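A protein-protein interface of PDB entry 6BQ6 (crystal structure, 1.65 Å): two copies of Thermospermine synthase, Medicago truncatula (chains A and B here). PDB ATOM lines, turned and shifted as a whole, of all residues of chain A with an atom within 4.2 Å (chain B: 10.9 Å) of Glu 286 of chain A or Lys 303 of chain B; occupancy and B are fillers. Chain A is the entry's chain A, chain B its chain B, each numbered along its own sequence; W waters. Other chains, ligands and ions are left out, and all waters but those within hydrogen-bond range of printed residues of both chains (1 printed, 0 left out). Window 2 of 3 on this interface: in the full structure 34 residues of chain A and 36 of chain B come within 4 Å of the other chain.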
ATOM      1  N   ARG A 121      33.338  19.705  13.232  1.00  0.00           N
ATOM      2  CA  ARG A 121      32.583  20.149  14.424  1.00  0.00           C
ATOM      3  C   ARG A 121      32.898  19.386  15.716  1.00  0.00           C
ATOM      4  O   ARG A 121      32.514  19.818  16.820  1.00  0.00           O
ATOM      5  CB  ARG A 121      31.086  20.073  14.163  1.00  0.00           C
ATOM      6  CG  ARG A 121      30.629  20.979  13.040  1.00  0.00           C
ATOM      7  CD  ARG A 121      29.146  20.870  12.736  1.00  0.00           C
ATOM      8  NE  ARG A 121      28.322  21.064  13.939  1.00  0.00           N
ATOM      9  CZ  ARG A 121      27.176  20.432  14.180  1.00  0.00           C
ATOM     10  NH1 ARG A 121      26.657  19.582  13.314  1.00  0.00           N
ATOM     11  NH2 ARG A 121      26.527  20.684  15.298  1.00  0.00           N
ATOM     12  N   ARG A 280      26.235  16.955  23.117  1.00  0.00           N
ATOM     13  CA  ARG A 280      26.419  18.211  23.859  1.00  0.00           C
ATOM     14  C   ARG A 280      27.883  18.419  24.278  1.00  0.00           C
ATOM     15  O   ARG A 280      28.420  19.536  24.190  1.00  0.00           O
ATOM     16  CB  ARG A 280      25.455  18.265  25.051  1.00  0.00           C
ATOM     17  CG  ARG A 280      25.471  19.588  25.825  1.00  0.00           C
ATOM     18  CD  ARG A 280      24.858  20.778  25.058  1.00  0.00           C
ATOM     19  NE  ARG A 280      23.392  20.685  24.904  1.00  0.00           N
ATOM     20  CZ  ARG A 280      22.470  21.259  25.700  1.00  0.00           C
ATOM     21  NH1 ARG A 280      22.807  22.021  26.746  1.00  0.00           N
ATOM     22  NH2 ARG A 280      21.176  21.078  25.430  1.00  0.00           N
ATOM     23  N   GLU A 285      28.098  23.569  18.494  1.00  0.00           N
ATOM     24  CA  GLU A 285      26.771  24.007  18.028  1.00  0.00           C
ATOM     25  C   GLU A 285      25.777  22.834  17.971  1.00  0.00           C
ATOM     26  O   GLU A 285      26.144  21.672  18.178  1.00  0.00           O
ATOM     27  CB  GLU A 285      26.855  24.680  16.653  1.00  0.00           C
ATOM     28  CG  GLU A 285      27.662  25.974  16.610  1.00  0.00           C
ATOM     29  CD  GLU A 285      27.609  26.619  15.230  1.00  0.00           C
ATOM     30  OE1 GLU A 285      27.769  25.890  14.229  1.00  0.00           O
ATOM     31  OE2 GLU A 285      27.391  27.840  15.128  1.00  0.00           O
ATOM     32  N   GLU A 286      24.531  23.153  17.678  1.00  0.00           N
ATOM     33  CA  GLU A 286      23.459  22.165  17.680  1.00  0.00           C
ATOM     34  C   GLU A 286      23.319  21.469  16.337  1.00  0.00           C
ATOM     35  O   GLU A 286      23.220  22.103  15.298  1.00  0.00           O
ATOM     36  CB  GLU A 286      22.116  22.821  18.034  1.00  0.00           C
ATOM     37  CG  GLU A 286      21.955  23.127  19.515  1.00  0.00           C
ATOM     38  CD  GLU A 286      21.496  21.907  20.306  1.00  0.00           C
ATOM     39  OE1 GLU A 286      20.395  21.351  19.973  1.00  0.00           O
ATOM     40  OE2 GLU A 286      22.234  21.509  21.257  1.00  0.00           O
ATOM     41  N   ASN A 287      23.253  20.141  16.346  1.00  0.00           N
ATOM     42  CA  ASN A 287      22.825  19.458  15.140  1.00  0.00           C
ATOM     43  C   ASN A 287      21.416  19.907  14.720  1.00  0.00           C
ATOM     44  O   ASN A 287      20.601  20.287  15.566  1.00  0.00           O
ATOM     45  CB  ASN A 287      22.787  17.952  15.340  1.00  0.00           C
ATOM     46  CG  ASN A 287      24.166  17.339  15.450  1.00  0.00           C
ATOM     47  OD1 ASN A 287      25.167  17.968  15.137  1.00  0.00           O
ATOM     48  ND2 ASN A 287      24.213  16.081  15.869  1.00  0.00           N
ATOM     49  N   ARG A 288      21.183  19.897  13.415  1.00  0.00           N
ATOM     50  CA  ARG A 288      19.886  20.300  12.840  1.00  0.00           C
ATOM     51  C   ARG A 288      18.972  19.091  12.707  1.00  0.00           C
ATOM     52  O   ARG A 288      17.756  19.187  12.956  1.00  0.00           O
ATOM     53  CB  ARG A 288      20.122  20.966  11.476  1.00  0.00           C
ATOM     54  CG  ARG A 288      20.902  22.267  11.557  1.00  0.00           C
ATOM     55  CD  ARG A 288      20.471  23.284  10.520  1.00  0.00           C
ATOM     56  NE  ARG A 288      21.171  23.130   9.234  1.00  0.00           N
ATOM     57  CZ  ARG A 288      20.625  23.232   8.009  1.00  0.00           C
ATOM     58  NH1 ARG A 288      21.373  23.108   6.920  1.00  0.00           N
ATOM     59  NH2 ARG A 288      19.296  23.432   7.874  1.00  0.00           N
ATOM     60  N   TYR A 289      19.544  17.954  12.296  1.00  0.00           N
ATOM     61  CA  TYR A 289      18.747  16.749  12.037  1.00  0.00           C
ATOM     62  C   TYR A 289      18.786  15.736  13.164  1.00  0.00           C
ATOM     63  O   TYR A 289      17.750  15.187  13.556  1.00  0.00           O
ATOM     64  CB  TYR A 289      19.181  15.998  10.745  1.00  0.00           C
ATOM     65  CG  TYR A 289      18.332  14.789  10.488  1.00  0.00           C
ATOM     66  CD1 TYR A 289      17.020  14.923  10.068  1.00  0.00           C
ATOM     67  CD2 TYR A 289      18.838  13.493  10.700  1.00  0.00           C
ATOM     68  CE1 TYR A 289      16.230  13.787   9.825  1.00  0.00           C
ATOM     69  CE2 TYR A 289      18.058  12.380  10.483  1.00  0.00           C
ATOM     70  CZ  TYR A 289      16.785  12.523  10.077  1.00  0.00           C
ATOM     71  OH  TYR A 289      16.036  11.403   9.889  1.00  0.00           O
ATOM     72  N   ASP A 291      19.353  13.914  16.725  1.00  0.00           N
ATOM     73  CA  ASP A 291      19.531  13.713  18.153  1.00  0.00           C
ATOM     74  C   ASP A 291      19.536  12.203  18.442  1.00  0.00           C
ATOM     75  O   ASP A 291      19.480  11.393  17.509  1.00  0.00           O
ATOM     76  CB  ASP A 291      18.498  14.498  18.979  1.00  0.00           C
ATOM     77  CG  ASP A 291      17.095  14.058  18.755  1.00  0.00           C
ATOM     78  OD1 ASP A 291      16.866  13.039  18.078  1.00  0.00           O
ATOM     79  OD2 ASP A 291      16.182  14.762  19.254  1.00  0.00           O
ATOM     80  N   THR A 294      16.583  10.250  17.285  1.00  0.00           N
ATOM     81  CA  THR A 294      16.573  10.177  15.824  1.00  0.00           C
ATOM     82  C   THR A 294      17.480   9.018  15.373  1.00  0.00           C
ATOM     83  O   THR A 294      17.096   8.239  14.522  1.00  0.00           O
ATOM     84  CB  THR A 294      17.010  11.492  15.145  1.00  0.00           C
ATOM     85  OG1 THR A 294      16.160  12.601  15.577  1.00  0.00           O
ATOM     86  CG2 THR A 294      16.927  11.359  13.635  1.00  0.00           C
ATOM     87  N   ALA B 221       4.731  13.951   5.623  1.00  0.00           N
ATOM     88  CA  ALA B 221       5.434  14.039   6.912  1.00  0.00           C
ATOM     89  C   ALA B 221       6.968  14.117   6.753  1.00  0.00           C
ATOM     90  O   ALA B 221       7.729  13.714   7.626  1.00  0.00           O
ATOM     91  CB  ALA B 221       5.007  12.950   7.832  1.00  0.00           C
ATOM     92  N   GLY B 222       7.379  14.700   5.646  1.00  0.00           N
ATOM     93  CA  GLY B 222       8.806  14.986   5.403  1.00  0.00           C
ATOM     94  C   GLY B 222       9.389  16.086   6.280  1.00  0.00           C
ATOM     95  O   GLY B 222       8.700  16.847   6.951  1.00  0.00           O
ATOM     96  N   ILE B 223      10.725  16.119   6.286  1.00  0.00           N
ATOM     97  CA  ILE B 223      11.457  17.063   7.158  1.00  0.00           C
ATOM     98  C   ILE B 223      10.950  18.494   6.981  1.00  0.00           C
ATOM     99  O   ILE B 223      10.847  19.229   7.972  1.00  0.00           O
ATOM    100  CB  ILE B 223      12.980  16.905   6.917  1.00  0.00           C
ATOM    101  CG1 ILE B 223      13.844  17.867   7.721  1.00  0.00           C
ATOM    102  CG2 ILE B 223      13.326  17.135   5.468  1.00  0.00           C
ATOM    103  CD1 ILE B 223      13.603  17.797   9.182  1.00  0.00           C
ATOM    104  N   PHE B 224      10.667  18.911   5.745  1.00  0.00           N
ATOM    105  CA  PHE B 224      10.009  20.187   5.486  1.00  0.00           C
ATOM    106  C   PHE B 224       8.515  20.073   5.144  1.00  0.00           C
ATOM    107  O   PHE B 224       7.723  20.969   5.491  1.00  0.00           O
ATOM    108  CB  PHE B 224      10.787  20.951   4.414  1.00  0.00           C
ATOM    109  CG  PHE B 224      12.207  21.185   4.822  1.00  0.00           C
ATOM    110  CD1 PHE B 224      12.503  21.879   6.014  1.00  0.00           C
ATOM    111  CD2 PHE B 224      13.230  20.634   4.112  1.00  0.00           C
ATOM    112  CE1 PHE B 224      13.818  22.075   6.399  1.00  0.00           C
ATOM    113  CE2 PHE B 224      14.552  20.809   4.493  1.00  0.00           C
ATOM    114  CZ  PHE B 224      14.845  21.501   5.648  1.00  0.00           C
ATOM    115  N   HIS B 226       6.216  18.265   6.246  1.00  0.00           N
ATOM    116  CA  HIS B 226       5.325  17.980   7.396  1.00  0.00           C
ATOM    117  C   HIS B 226       4.573  19.229   7.903  1.00  0.00           C
ATOM    118  O   HIS B 226       3.594  19.113   8.638  1.00  0.00           O
ATOM    119  CB  HIS B 226       6.063  17.349   8.592  1.00  0.00           C
ATOM    120  CG  HIS B 226       6.853  18.341   9.403  1.00  0.00           C
ATOM    121  ND1 HIS B 226       8.150  18.697   9.090  1.00  0.00           N
ATOM    122  CD2 HIS B 226       6.510  19.086  10.484  1.00  0.00           C
ATOM    123  CE1 HIS B 226       8.562  19.640   9.932  1.00  0.00           C
ATOM    124  NE2 HIS B 226       7.589  19.879  10.789  1.00  0.00           N
ATOM    125  N   PHE B 230       0.502  17.920   8.421  1.00  0.00           N
ATOM    126  CA  PHE B 230       0.778  16.933   9.489  1.00  0.00           C
ATOM    127  C   PHE B 230       0.886  17.594  10.844  1.00  0.00           C
ATOM    128  O   PHE B 230       0.220  17.186  11.806  1.00  0.00           O
ATOM    129  CB  PHE B 230       2.070  16.186   9.132  1.00  0.00           C
ATOM    130  CG  PHE B 230       2.510  15.115  10.096  1.00  0.00           C
ATOM    131  CD1 PHE B 230       1.796  13.940  10.257  1.00  0.00           C
ATOM    132  CD2 PHE B 230       3.707  15.214  10.776  1.00  0.00           C
ATOM    133  CE1 PHE B 230       2.244  12.927  11.096  1.00  0.00           C
ATOM    134  CE2 PHE B 230       4.173  14.181  11.589  1.00  0.00           C
ATOM    135  CZ  PHE B 230       3.448  13.018  11.740  1.00  0.00           C
ATOM    136  N   SER B 248       5.004   8.128  11.214  1.00  0.00           N
ATOM    137  CA  SER B 248       5.236   8.291   9.789  1.00  0.00           C
ATOM    138  C   SER B 248       6.028   7.160   9.163  1.00  0.00           C
ATOM    139  O   SER B 248       6.692   6.383   9.865  1.00  0.00           O
ATOM    140  CB  SER B 248       5.925   9.641   9.537  1.00  0.00           C
ATOM    141  OG  SER B 248       7.237   9.667  10.115  1.00  0.00           O
ATOM    142  N   SER B 297       9.633   2.667  15.718  1.00  0.00           N
ATOM    143  CA  SER B 297      10.506   3.506  14.860  1.00  0.00           C
ATOM    144  C   SER B 297       9.684   4.625  14.188  1.00  0.00           C
ATOM    145  O   SER B 297      10.046   5.812  14.251  1.00  0.00           O
ATOM    146  CB  SER B 297      11.164   2.648  13.769  1.00  0.00           C
ATOM    147  OG  SER B 297      11.978   3.498  12.911  1.00  0.00           O
ATOM    148  N   SER B 298       8.538   4.248  13.624  1.00  0.00           N
ATOM    149  CA  SER B 298       7.625   5.208  12.973  1.00  0.00           C
ATOM    150  C   SER B 298       7.164   6.298  13.891  1.00  0.00           C
ATOM    151  O   SER B 298       6.957   7.438  13.444  1.00  0.00           O
ATOM    152  CB  SER B 298       6.369   4.531  12.408  1.00  0.00           C
ATOM    153  OG  SER B 298       6.770   3.741  11.282  1.00  0.00           O
ATOM    154  N   SER B 299       6.945   5.946  15.149  1.00  0.00           N
ATOM    155  CA  SER B 299       6.444   6.897  16.139  1.00  0.00           C
ATOM    156  C   SER B 299       7.538   7.709  16.851  1.00  0.00           C
ATOM    157  O   SER B 299       7.264   8.499  17.733  1.00  0.00           O
ATOM    158  CB  SER B 299       5.481   6.196  17.086  1.00  0.00           C
ATOM    159  OG  SER B 299       6.151   5.251  17.836  1.00  0.00           O
ATOM    160  N   THR B 300       8.778   7.507  16.451  1.00  0.00           N
ATOM    161  CA  THR B 300       9.880   8.301  16.945  1.00  0.00           C
ATOM    162  C   THR B 300      10.224   9.212  15.800  1.00  0.00           C
ATOM    163  O   THR B 300      10.945   8.825  14.868  1.00  0.00           O
ATOM    164  CB  THR B 300      11.113   7.419  17.271  1.00  0.00           C
ATOM    165  OG1 THR B 300      10.756   6.341  18.171  1.00  0.00           O
ATOM    166  CG2 THR B 300      12.227   8.285  17.857  1.00  0.00           C
ATOM    167  N   LEU B 301       9.771  10.430  15.876  1.00  0.00           N
ATOM    168  CA  LEU B 301       9.973  11.365  14.777  1.00  0.00           C
ATOM    169  C   LEU B 301      11.388  11.942  14.929  1.00  0.00           C
ATOM    170  O   LEU B 301      11.992  11.823  15.994  1.00  0.00           O
ATOM    171  CB  LEU B 301       8.937  12.470  14.852  1.00  0.00           C
ATOM    172  CG  LEU B 301       7.538  11.849  14.735  1.00  0.00           C
ATOM    173  CD1 LEU B 301       6.537  12.931  14.852  1.00  0.00           C
ATOM    174  CD2 LEU B 301       7.405  11.087  13.436  1.00  0.00           C
ATOM    175  N   SER B 302      11.909  12.580  13.894  1.00  0.00           N
ATOM    176  CA  SER B 302      13.269  13.158  13.977  1.00  0.00           C
ATOM    177  C   SER B 302      13.246  14.427  14.812  1.00  0.00           C
ATOM    178  O   SER B 302      12.204  14.998  15.081  1.00  0.00           O
ATOM    179  CB  SER B 302      13.812  13.478  12.601  1.00  0.00           C
ATOM    180  OG  SER B 302      13.181  14.631  12.037  1.00  0.00           O
ATOM    181  N   LYS B 303      14.430  14.902  15.188  1.00  0.00           N
ATOM    182  CA  LYS B 303      14.542  16.067  16.067  1.00  0.00           C
ATOM    183  C   LYS B 303      13.732  17.267  15.594  1.00  0.00           C
ATOM    184  O   LYS B 303      12.980  17.864  16.375  1.00  0.00           O
ATOM    185  CB  LYS B 303      16.023  16.473  16.184  1.00  0.00           C
ATOM    186  CG  LYS B 303      16.277  17.672  17.075  1.00  0.00           C
ATOM    187  CD  LYS B 303      17.706  18.134  16.967  1.00  0.00           C
ATOM    188  CE  LYS B 303      18.014  19.209  18.003  1.00  0.00           C
ATOM    189  NZ  LYS B 303      19.471  19.433  17.984  1.00  0.00           N
ATOM    190  N   ALA B 304      13.911  17.630  14.324  1.00  0.00           N
ATOM    191  CA  ALA B 304      13.279  18.814  13.759  1.00  0.00           C
ATOM    192  C   ALA B 304      11.753  18.678  13.688  1.00  0.00           C
ATOM    193  O   ALA B 304      10.993  19.627  13.929  1.00  0.00           O
ATOM    194  CB  ALA B 304      13.813  19.016  12.381  1.00  0.00           C
ATOM    195  N   VAL B 305      11.310  17.488  13.308  1.00  0.00           N
ATOM    196  CA  VAL B 305       9.863  17.251  13.161  1.00  0.00           C
ATOM    197  C   VAL B 305       9.215  17.205  14.528  1.00  0.00           C
ATOM    198  O   VAL B 305       8.180  17.846  14.765  1.00  0.00           O
ATOM    199  CB  VAL B 305       9.576  15.954  12.341  1.00  0.00           C
ATOM    200  CG1 VAL B 305       8.082  15.664  12.281  1.00  0.00           C
ATOM    201  CG2 VAL B 305      10.121  16.051  10.942  1.00  0.00           C
ATOM    202  N   ARG B 306       9.842  16.509  15.475  1.00  0.00           N
ATOM    203  CA  ARG B 306       9.359  16.507  16.864  1.00  0.00           C
ATOM    204  C   ARG B 306       9.189  17.937  17.405  1.00  0.00           C
ATOM    205  O   ARG B 306       8.170  18.304  17.954  1.00  0.00           O
ATOM    206  CB  ARG B 306      10.318  15.737  17.757  1.00  0.00           C
ATOM    207  CG  ARG B 306       9.677  14.839  18.749  1.00  0.00           C
ATOM    208  CD  ARG B 306      10.650  13.989  19.561  1.00  0.00           C
ATOM    209  NE  ARG B 306      11.668  13.301  18.726  1.00  0.00           N
ATOM    210  CZ  ARG B 306      12.990  13.518  18.774  1.00  0.00           C
ATOM    211  NH1 ARG B 306      13.535  14.362  19.659  1.00  0.00           N
ATOM    212  NH2 ARG B 306      13.787  12.852  17.927  1.00  0.00           N
ATOM    213  N   ASN B 307      10.185  18.763  17.210  1.00  0.00           N
ATOM    214  CA  ASN B 307      10.123  20.109  17.769  1.00  0.00           C
ATOM    215  C   ASN B 307       9.101  20.990  17.051  1.00  0.00           C
ATOM    216  O   ASN B 307       8.385  21.804  17.689  1.00  0.00           O
ATOM    217  CB  ASN B 307      11.523  20.689  17.789  1.00  0.00           C
ATOM    218  CG  ASN B 307      12.433  19.976  18.822  1.00  0.00           C
ATOM    219  OD1 ASN B 307      11.950  19.251  19.712  1.00  0.00           O
ATOM    220  ND2 ASN B 307      13.740  20.198  18.724  1.00  0.00           N
ATOM    221  N   SER B 308       9.011  20.812  15.734  1.00  0.00           N
ATOM    222  CA  SER B 308       8.034  21.520  14.910  1.00  0.00           C
ATOM    223  C   SER B 308       6.604  21.177  15.342  1.00  0.00           C
ATOM    224  O   SER B 308       5.753  22.085  15.532  1.00  0.00           O
ATOM    225  CB  SER B 308       8.328  21.212  13.434  1.00  0.00           C
ATOM    226  OG  SER B 308       7.401  21.776  12.549  1.00  0.00           O
ATOM    227  N   LEU B 309       6.344  19.891  15.557  1.00  0.00           N
ATOM    228  CA  LEU B 309       5.031  19.460  16.093  1.00  0.00           C
ATOM    229  C   LEU B 309       4.735  20.045  17.462  1.00  0.00           C
ATOM    230  O   LEU B 309       3.653  20.570  17.679  1.00  0.00           O
ATOM    231  CB  LEU B 309       4.894  17.934  16.110  1.00  0.00           C
ATOM    232  CG  LEU B 309       4.126  17.425  14.882  1.00  0.00           C
ATOM    233  CD1 LEU B 309       4.759  17.760  13.558  1.00  0.00           C
ATOM    234  CD2 LEU B 309       3.917  15.926  15.002  1.00  0.00           C
ATOM    235  N   ASN B 310       5.717  19.976  18.359  1.00  0.00           N
ATOM    236  CA  ASN B 310       5.595  20.549  19.691  1.00  0.00           C
ATOM    237  C   ASN B 310       5.211  22.012  19.698  1.00  0.00           C
ATOM    238  O   ASN B 310       4.348  22.408  20.487  1.00  0.00           O
ATOM    239  CB  ASN B 310       6.909  20.412  20.460  1.00  0.00           C
ATOM    240  CG  ASN B 310       6.918  19.224  21.379  1.00  0.00           C
ATOM    241  OD1 ASN B 310       7.809  18.354  21.295  1.00  0.00           O
ATOM    242  ND2 ASN B 310       5.947  19.195  22.318  1.00  0.00           N
ATOM    243  N   ASN B 311       5.810  22.796  18.798  1.00  0.00           N
ATOM    244  CA  ASN B 311       5.631  24.253  18.780  1.00  0.00           C
ATOM    245  C   ASN B 311       4.483  24.749  17.893  1.00  0.00           C
ATOM    246  O   ASN B 311       4.182  25.952  17.863  1.00  0.00           O
ATOM    247  CB  ASN B 311       6.950  24.925  18.382  1.00  0.00           C
ATOM    248  CG  ASN B 311       8.075  24.555  19.316  1.00  0.00           C
ATOM    249  OD1 ASN B 311       7.870  24.392  20.520  1.00  0.00           O
ATOM    250  ND2 ASN B 311       9.256  24.372  18.766  1.00  0.00           N
HETATM  251  O   HOH W   1      15.387  16.311  12.385  1.00  0.00           O
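The side-chain carboxylate (OD2) of Asp 291 of chain A lies within salt-bridge range of the guanidinium group (NH1) of Arg 306 of chain B (2.7 Å). The side-chain amino group (NZ) of Lys 303 of chain B sits at hydrogen-bond distance from the backbone carbonyl oxygen (O) of Asn 287 of chain A, at 2.8 Å. The side-chain carboxylate of Glu 286 of chain A lies within salt-bridge range of the side-chain amino group of Lys 303 of chain B (2.9 Å). The side-chain hydroxyl (OG1) of Thr 294 of chain A lies within hydrogen-bond range of the guanidinium group (NH2) of Arg 306 of chain B, 3.3 Å away. OG1 of Thr 294 of chain A sits at hydrogen-bond distance from N of Lys 303 of chain B (2.9 Å).
Of the 22 printed residues of chain B, 4 touch a printed residue of chain A. Printed residues of chain B that touch a printed residue of chain A: Ser 302, Lys 303, Ala 304 and Arg 306. Hydrophobic or aromatic side chains of chain B within 4 Å of the printed part of chain A: Ala 304.
Glu 285 of chain A touches none of the printed residues of chain B. Asn 287 of chain A touches just one residue of chain B: Lys 303. Of the printed residues of chain B, Arg 288 of chain A touches Ala 304 (3.99 Å). Tyr 289 of chain A touches just these residues of chain B: Ser 302 and Lys 303. Asp 291 of chain A touches just these residues of chain B: Lys 303 (3.5 Å) and Arg 306 (2.7 Å). Of the printed residues of chain B, Thr 294 of chain A touches Ser 302 (3.4 Å), Lys 303 (2.9 Å) and Arg 306 (3.3 Å). Phe 224 of chain B touches none of the printed residues of chain A. Printed residues of chain A within 4 Å of Ser 302 of chain B: Tyr 289 and Thr 294. Of the printed residues of chain A, Ala 304 of chain B touches Arg 288. Printed residues of chain A within 4 Å of Arg 306 of chain B: Asp 291 (2.7 Å) and Thr 294 (3.3 Å). The nearest residue of chain B that does not touch Glu 286 of chain A is Asn 307 of chain B (6.9 Å). The nearest residue of chain A that does not touch Lys 303 of chain B is Arg 288 of chain A (4.1 Å).
Water W1 lies within hydrogen-bond range of N of Ala 304 of chain B (2.8 Å), OG of Ser 302 of chain B (2.8 Å), O of Tyr 289 of chain A (2.9 Å) and N of Lys 303 of chain B (3.3 Å).
No position is printed for both chains. Of the 10 pairs that touch across the chains among the printed residues, none has its exchanged pair printed and touching as well.
Among the printed residues, pairs that only touch across the chains: Thr 294 of chain A with Ser 302 of chain B, Tyr 289 of chain A with Lys 303 of chain B, Asp 291 of chain A with Lys 303 of chain B, Tyr 289 of chain A with Ser 302 of chain B and Arg 288 of chain A with Ala 304 of chain B.
The guanidinium group (NH2) of Arg 306 of chain B sits at hydrogen-bond distance from the backbone carbonyl oxygen (O) of Leu 301 of chain B (2.8 Å). The side-chain carboxylate (OE2) of Glu 286 of chain A is in salt-bridge range of the guanidinium group (NE) of Arg 280 of chain A (3.9 Å). The side-chain carboxylate of Asp 291 of chain A lies within hydrogen-bond range of the side-chain hydroxyl of Thr 294 of chain A (2.6 Å). The backbone carbonyl oxygen (O) of Arg 306 of chain B lies close to the side-chain amide oxygen (OD1) of Asn 310 of chain B, 3.4 Å away. ND2 of Asn 307 of chain B sits close to O of Lys 303 of chain B. The guanidinium group (NH1) of Arg 121 of chain A lies within hydrogen-bond range of the side-chain amide oxygen (OD1) of Asn 287 of chain A (2.9 Å).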
